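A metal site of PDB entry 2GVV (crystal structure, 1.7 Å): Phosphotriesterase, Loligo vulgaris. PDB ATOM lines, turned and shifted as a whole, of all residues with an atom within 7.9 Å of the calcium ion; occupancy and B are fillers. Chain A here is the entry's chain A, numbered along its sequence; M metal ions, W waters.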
ATOM      1  N   GLU A  21     -12.790   8.853  22.884  1.00  0.00           N
ATOM      2  CA  GLU A  21     -13.509  10.025  22.416  1.00  0.00           C
ATOM      3  C   GLU A  21     -13.408  10.231  20.910  1.00  0.00           C
ATOM      4  O   GLU A  21     -12.808   9.426  20.199  1.00  0.00           O
ATOM      5  CB  GLU A  21     -12.937  11.262  23.139  1.00  0.00           C
ATOM      6  CG  GLU A  21     -13.821  11.818  24.246  1.00  0.00           C
ATOM      7  CD  GLU A  21     -14.807  12.842  23.730  1.00  0.00           C
ATOM      8  OE1 GLU A  21     -15.219  12.722  22.555  1.00  0.00           O
ATOM      9  OE2 GLU A  21     -15.184  13.754  24.501  1.00  0.00           O
ATOM     10  N   GLY A  22     -14.016  11.320  20.448  1.00  0.00           N
ATOM     11  CA  GLY A  22     -14.000  11.712  19.053  1.00  0.00           C
ATOM     12  C   GLY A  22     -14.122  10.665  17.956  1.00  0.00           C
ATOM     13  O   GLY A  22     -13.286  10.623  17.052  1.00  0.00           O
ATOM     14  N   PRO A  23     -15.147   9.803  18.003  1.00  0.00           N
ATOM     15  CA  PRO A  23     -15.277   8.793  16.944  1.00  0.00           C
ATOM     16  C   PRO A  23     -15.562   9.486  15.608  1.00  0.00           C
ATOM     17  O   PRO A  23     -16.321  10.454  15.539  1.00  0.00           O
ATOM     18  CB  PRO A  23     -16.439   7.934  17.432  1.00  0.00           C
ATOM     19  CG  PRO A  23     -17.284   8.913  18.225  1.00  0.00           C
ATOM     20  CD  PRO A  23     -16.245   9.689  18.985  1.00  0.00           C
ATOM     21  N   VAL A  24     -14.927   9.000  14.552  1.00  0.00           N
ATOM     22  CA  VAL A  24     -15.108   9.620  13.247  1.00  0.00           C
ATOM     23  C   VAL A  24     -14.771   8.649  12.113  1.00  0.00           C
ATOM     24  O   VAL A  24     -13.981   7.728  12.292  1.00  0.00           O
ATOM     25  CB  VAL A  24     -14.208  10.866  13.121  1.00  0.00           C
ATOM     26  CG1 VAL A  24     -12.733  10.447  13.127  1.00  0.00           C
ATOM     27  CG2 VAL A  24     -14.535  11.640  11.850  1.00  0.00           C
ATOM     28  N   PHE A  25     -15.383   8.873  10.955  1.00  0.00           N
ATOM     29  CA  PHE A  25     -15.130   8.059   9.769  1.00  0.00           C
ATOM     30  C   PHE A  25     -14.510   8.979   8.731  1.00  0.00           C
ATOM     31  O   PHE A  25     -14.933  10.123   8.593  1.00  0.00           O
ATOM     32  CB  PHE A  25     -16.441   7.474   9.218  1.00  0.00           C
ATOM     33  CG  PHE A  25     -16.923   6.256   9.945  1.00  0.00           C
ATOM     34  CD1 PHE A  25     -16.446   4.990   9.617  1.00  0.00           C
ATOM     35  CD2 PHE A  25     -17.865   6.374  10.968  1.00  0.00           C
ATOM     36  CE1 PHE A  25     -16.881   3.854  10.292  1.00  0.00           C
ATOM     37  CE2 PHE A  25     -18.314   5.236  11.648  1.00  0.00           C
ATOM     38  CZ  PHE A  25     -17.823   3.971  11.315  1.00  0.00           C
ATOM     39  N   CYS A  76     -12.969  15.040  16.829  1.00  0.00           N
ATOM     40  CA  CYS A  76     -12.574  14.991  15.419  1.00  0.00           C
ATOM     41  C   CYS A  76     -13.675  15.307  14.409  1.00  0.00           C
ATOM     42  O   CYS A  76     -14.856  15.146  14.682  1.00  0.00           O
ATOM     43  CB  CYS A  76     -12.048  13.596  15.072  1.00  0.00           C
ATOM     44  SG  CYS A  76     -10.764  12.924  16.144  1.00  0.00           S
ATOM     45  N   GLN A  77     -13.230  15.728  13.228  1.00  0.00           N
ATOM     46  CA  GLN A  77     -14.087  15.999  12.075  1.00  0.00           C
ATOM     47  C   GLN A  77     -13.221  15.677  10.858  1.00  0.00           C
ATOM     48  O   GLN A  77     -12.027  15.977  10.859  1.00  0.00           O
ATOM     49  CB  GLN A  77     -14.509  17.471  12.009  1.00  0.00           C
ATOM     50  CG  GLN A  77     -15.665  17.861  12.931  1.00  0.00           C
ATOM     51  CD  GLN A  77     -16.966  17.174  12.569  1.00  0.00           C
ATOM     52  OE1 GLN A  77     -17.242  16.054  13.009  1.00  0.00           O
ATOM     53  NE2 GLN A  77     -17.756  17.833  11.748  1.00  0.00           N
ATOM     54  N   ASP A 121     -14.192  19.677  21.147  1.00  0.00           N
ATOM     55  CA  ASP A 121     -14.918  19.069  20.027  1.00  0.00           C
ATOM     56  C   ASP A 121     -15.102  20.093  18.920  1.00  0.00           C
ATOM     57  O   ASP A 121     -14.872  21.294  19.110  1.00  0.00           O
ATOM     58  CB  ASP A 121     -16.284  18.537  20.490  1.00  0.00           C
ATOM     59  CG  ASP A 121     -16.716  17.280  19.748  1.00  0.00           C
ATOM     60  OD1 ASP A 121     -16.151  16.983  18.671  1.00  0.00           O
ATOM     61  OD2 ASP A 121     -17.638  16.580  20.231  1.00  0.00           O
ATOM     62  N   CYS A 122     -15.506  19.638  17.743  1.00  0.00           N
ATOM     63  CA  CYS A 122     -15.701  20.554  16.630  1.00  0.00           C
ATOM     64  C   CYS A 122     -16.709  20.018  15.637  1.00  0.00           C
ATOM     65  O   CYS A 122     -16.968  18.812  15.584  1.00  0.00           O
ATOM     66  CB  CYS A 122     -14.365  20.827  15.930  1.00  0.00           C
ATOM     67  SG  CYS A 122     -13.444  19.356  15.406  1.00  0.00           S
ATOM     68  N   ILE A 177     -20.784  20.015  20.252  1.00  0.00           N
ATOM     69  CA  ILE A 177     -21.203  21.107  19.394  1.00  0.00           C
ATOM     70  C   ILE A 177     -21.751  20.525  18.096  1.00  0.00           C
ATOM     71  O   ILE A 177     -21.302  19.473  17.638  1.00  0.00           O
ATOM     72  CB  ILE A 177     -19.999  22.059  19.112  1.00  0.00           C
ATOM     73  CG1 ILE A 177     -20.452  23.259  18.286  1.00  0.00           C
ATOM     74  CG2 ILE A 177     -18.884  21.295  18.404  1.00  0.00           C
ATOM     75  CD1 ILE A 177     -19.425  24.390  18.264  1.00  0.00           C
ATOM     76  N   GLY A 230     -20.840  14.648  23.881  1.00  0.00           N
ATOM     77  CA  GLY A 230     -20.892  14.726  22.427  1.00  0.00           C
ATOM     78  C   GLY A 230     -22.299  14.675  21.832  1.00  0.00           C
ATOM     79  O   GLY A 230     -23.226  14.184  22.474  1.00  0.00           O
ATOM     80  N   MET A 231     -22.446  15.168  20.599  1.00  0.00           N
ATOM     81  CA  MET A 231     -23.738  15.194  19.928  1.00  0.00           C
ATOM     82  C   MET A 231     -23.645  15.124  18.399  1.00  0.00           C
ATOM     83  O   MET A 231     -22.606  15.416  17.827  1.00  0.00           O
ATOM     84  CB  MET A 231     -24.489  16.472  20.300  1.00  0.00           C
ATOM     85  CG  MET A 231     -23.733  17.749  19.940  1.00  0.00           C
ATOM     86  SD  MET A 231     -24.592  19.286  20.385  1.00  0.00           S
ATOM     87  CE  MET A 231     -25.055  18.893  22.012  1.00  0.00           C
ATOM     88  N   ASP A 232     -24.758  14.768  17.768  1.00  0.00           N
ATOM     89  CA  ASP A 232     -24.856  14.692  16.316  1.00  0.00           C
ATOM     90  C   ASP A 232     -26.334  14.619  15.946  1.00  0.00           C
ATOM     91  O   ASP A 232     -27.161  14.182  16.750  1.00  0.00           O
ATOM     92  CB  ASP A 232     -24.144  13.458  15.739  1.00  0.00           C
ATOM     93  CG  ASP A 232     -22.711  13.742  15.304  1.00  0.00           C
ATOM     94  OD1 ASP A 232     -22.426  14.821  14.740  1.00  0.00           O
ATOM     95  OD2 ASP A 232     -21.862  12.858  15.519  1.00  0.00           O
ATOM     96  N   PHE A 233     -26.657  15.057  14.728  1.00  0.00           N
ATOM     97  CA  PHE A 233     -28.027  15.033  14.229  1.00  0.00           C
ATOM     98  C   PHE A 233     -28.302  13.790  13.380  1.00  0.00           C
ATOM     99  O   PHE A 233     -27.390  13.255  12.744  1.00  0.00           O
ATOM    100  CB  PHE A 233     -28.270  16.249  13.320  1.00  0.00           C
ATOM    101  CG  PHE A 233     -28.493  17.531  14.050  1.00  0.00           C
ATOM    102  CD1 PHE A 233     -29.696  17.771  14.708  1.00  0.00           C
ATOM    103  CD2 PHE A 233     -27.521  18.532  14.056  1.00  0.00           C
ATOM    104  CE1 PHE A 233     -29.931  18.985  15.350  1.00  0.00           C
ATOM    105  CE2 PHE A 233     -27.741  19.747  14.704  1.00  0.00           C
ATOM    106  CZ  PHE A 233     -28.951  19.965  15.352  1.00  0.00           C
ATOM    107  N   ASN A 272     -19.162  10.179  23.461  1.00  0.00           N
ATOM    108  CA  ASN A 272     -19.372  10.755  22.141  1.00  0.00           C
ATOM    109  C   ASN A 272     -19.911   9.707  21.191  1.00  0.00           C
ATOM    110  O   ASN A 272     -19.888   8.512  21.487  1.00  0.00           O
ATOM    111  CB  ASN A 272     -18.064  11.342  21.597  1.00  0.00           C
ATOM    112  CG  ASN A 272     -18.277  12.622  20.823  1.00  0.00           C
ATOM    113  OD1 ASN A 272     -19.284  12.784  20.139  1.00  0.00           O
ATOM    114  ND2 ASN A 272     -17.317  13.545  20.922  1.00  0.00           N
ATOM    115  N   LEU A 273     -20.376  10.147  20.022  1.00  0.00           N
ATOM    116  CA  LEU A 273     -20.943   9.219  19.061  1.00  0.00           C
ATOM    117  C   LEU A 273     -20.771   9.702  17.630  1.00  0.00           C
ATOM    118  O   LEU A 273     -20.393  10.842  17.390  1.00  0.00           O
ATOM    119  CB  LEU A 273     -22.426   9.030  19.384  1.00  0.00           C
ATOM    120  CG  LEU A 273     -23.270  10.310  19.502  1.00  0.00           C
ATOM    121  CD1 LEU A 273     -23.837  10.656  18.148  1.00  0.00           C
ATOM    122  CD2 LEU A 273     -24.408  10.090  20.499  1.00  0.00           C
ATOM    123  N   HIS A 274     -21.038   8.816  16.684  1.00  0.00           N
ATOM    124  CA  HIS A 274     -20.907   9.156  15.276  1.00  0.00           C
ATOM    125  C   HIS A 274     -21.624   8.089  14.460  1.00  0.00           C
ATOM    126  O   HIS A 274     -21.558   6.907  14.796  1.00  0.00           O
ATOM    127  CB  HIS A 274     -19.423   9.205  14.875  1.00  0.00           C
ATOM    128  CG  HIS A 274     -19.110  10.200  13.804  1.00  0.00           C
ATOM    129  ND1 HIS A 274     -19.140  11.565  14.026  1.00  0.00           N
ATOM    130  CD2 HIS A 274     -18.736  10.034  12.508  1.00  0.00           C
ATOM    131  CE1 HIS A 274     -18.798  12.189  12.911  1.00  0.00           C
ATOM    132  NE2 HIS A 274     -18.554  11.285  11.975  1.00  0.00           N
ATOM    133  N   PHE A 275     -22.305   8.509  13.398  1.00  0.00           N
ATOM    134  CA  PHE A 275     -23.002   7.557  12.533  1.00  0.00           C
ATOM    135  C   PHE A 275     -22.044   7.029  11.477  1.00  0.00           C
ATOM    136  O   PHE A 275     -21.148   7.743  11.037  1.00  0.00           O
ATOM    137  CB  PHE A 275     -24.155   8.222  11.777  1.00  0.00           C
ATOM    138  CG  PHE A 275     -25.378   8.468  12.602  1.00  0.00           C
ATOM    139  CD1 PHE A 275     -25.452   9.570  13.454  1.00  0.00           C
ATOM    140  CD2 PHE A 275     -26.487   7.640  12.480  1.00  0.00           C
ATOM    141  CE1 PHE A 275     -26.615   9.841  14.176  1.00  0.00           C
ATOM    142  CE2 PHE A 275     -27.655   7.889  13.201  1.00  0.00           C
ATOM    143  CZ  PHE A 275     -27.716   8.994  14.048  1.00  0.00           C
ATOM    144  N   PHE A 283     -21.914   4.612  16.432  1.00  0.00           N
ATOM    145  CA  PHE A 283     -20.816   4.135  17.236  1.00  0.00           C
ATOM    146  C   PHE A 283     -20.705   5.078  18.412  1.00  0.00           C
ATOM    147  O   PHE A 283     -20.683   6.298  18.241  1.00  0.00           O
ATOM    148  CB  PHE A 283     -19.516   4.102  16.435  1.00  0.00           C
ATOM    149  CG  PHE A 283     -19.460   2.997  15.419  1.00  0.00           C
ATOM    150  CD1 PHE A 283     -20.218   3.065  14.255  1.00  0.00           C
ATOM    151  CD2 PHE A 283     -18.695   1.865  15.662  1.00  0.00           C
ATOM    152  CE1 PHE A 283     -20.217   2.007  13.338  1.00  0.00           C
ATOM    153  CE2 PHE A 283     -18.684   0.800  14.750  1.00  0.00           C
ATOM    154  CZ  PHE A 283     -19.443   0.882  13.588  1.00  0.00           C
ATOM    155  N   GLN A 304     -22.382  14.308   7.153  1.00  0.00           N
ATOM    156  CA  GLN A 304     -21.323  15.157   7.690  1.00  0.00           C
ATOM    157  C   GLN A 304     -20.782  15.946   6.498  1.00  0.00           C
ATOM    158  O   GLN A 304     -21.043  15.601   5.344  1.00  0.00           O
ATOM    159  CB  GLN A 304     -20.187  14.310   8.276  1.00  0.00           C
ATOM    160  CG  GLN A 304     -20.505  13.613   9.589  1.00  0.00           C
ATOM    161  CD  GLN A 304     -20.391  14.555  10.775  1.00  0.00           C
ATOM    162  OE1 GLN A 304     -21.394  15.006  11.329  1.00  0.00           O
ATOM    163  NE2 GLN A 304     -19.159  14.867  11.158  1.00  0.00           N
HETATM  164 CA    CA M   1     -19.756  12.732  16.171  1.00  0.00          CA
HETATM  165  O   HOH W   1     -19.545  14.740  14.942  1.00  0.00           O
HETATM  166  O   HOH W   2     -20.111  14.019  17.958  1.00  0.00           O
HETATM  167  O   HOH W   3     -17.565  12.405  16.838  1.00  0.00           O
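The calcium ion is bound by OD2 of Asp 232 (2.2 Å), water W2 (2.2 Å), water W3 (2.3 Å), O of Leu 273 (2.3 Å), water W1 (2.4 Å) and ND1 of His 274 (2.5 Å).
The calcium ion has six donor atoms within binding distance.
A ring nitrogen (ND1) of His 274 sits close to the backbone carbonyl oxygen of Pro 23 (3.4 Å).
The backbone NH (N) of Phe 283 sits at hydrogen-bond distance from the backbone carbonyl oxygen (O) of His 274, 2.8 Å away.
ND2 of Asn 272 lies within hydrogen-bond range of OD2 of Asp 121 (3.1 Å).
The side-chain amide nitrogen of Asn 272 lies within hydrogen-bond range of the side-chain carboxylate of Glu 21.
Water W1 bridges OD1 of Asp 232 (2.9 Å) and OE1 of Gln 77 (3.3 Å).
Water W2 lies within hydrogen-bond range of OD1 of Asn 272 (2.6 Å) and O of Met 231 (2.9 Å).
Merely in contact with the calcium ion: Asn 272 (3.996 Å).
Of the 20 residues printed, 4 come within 4 Å of the calcium ion.
The nearest printed residue that does not touch the calcium ion is Pro 23 (4.2 Å).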
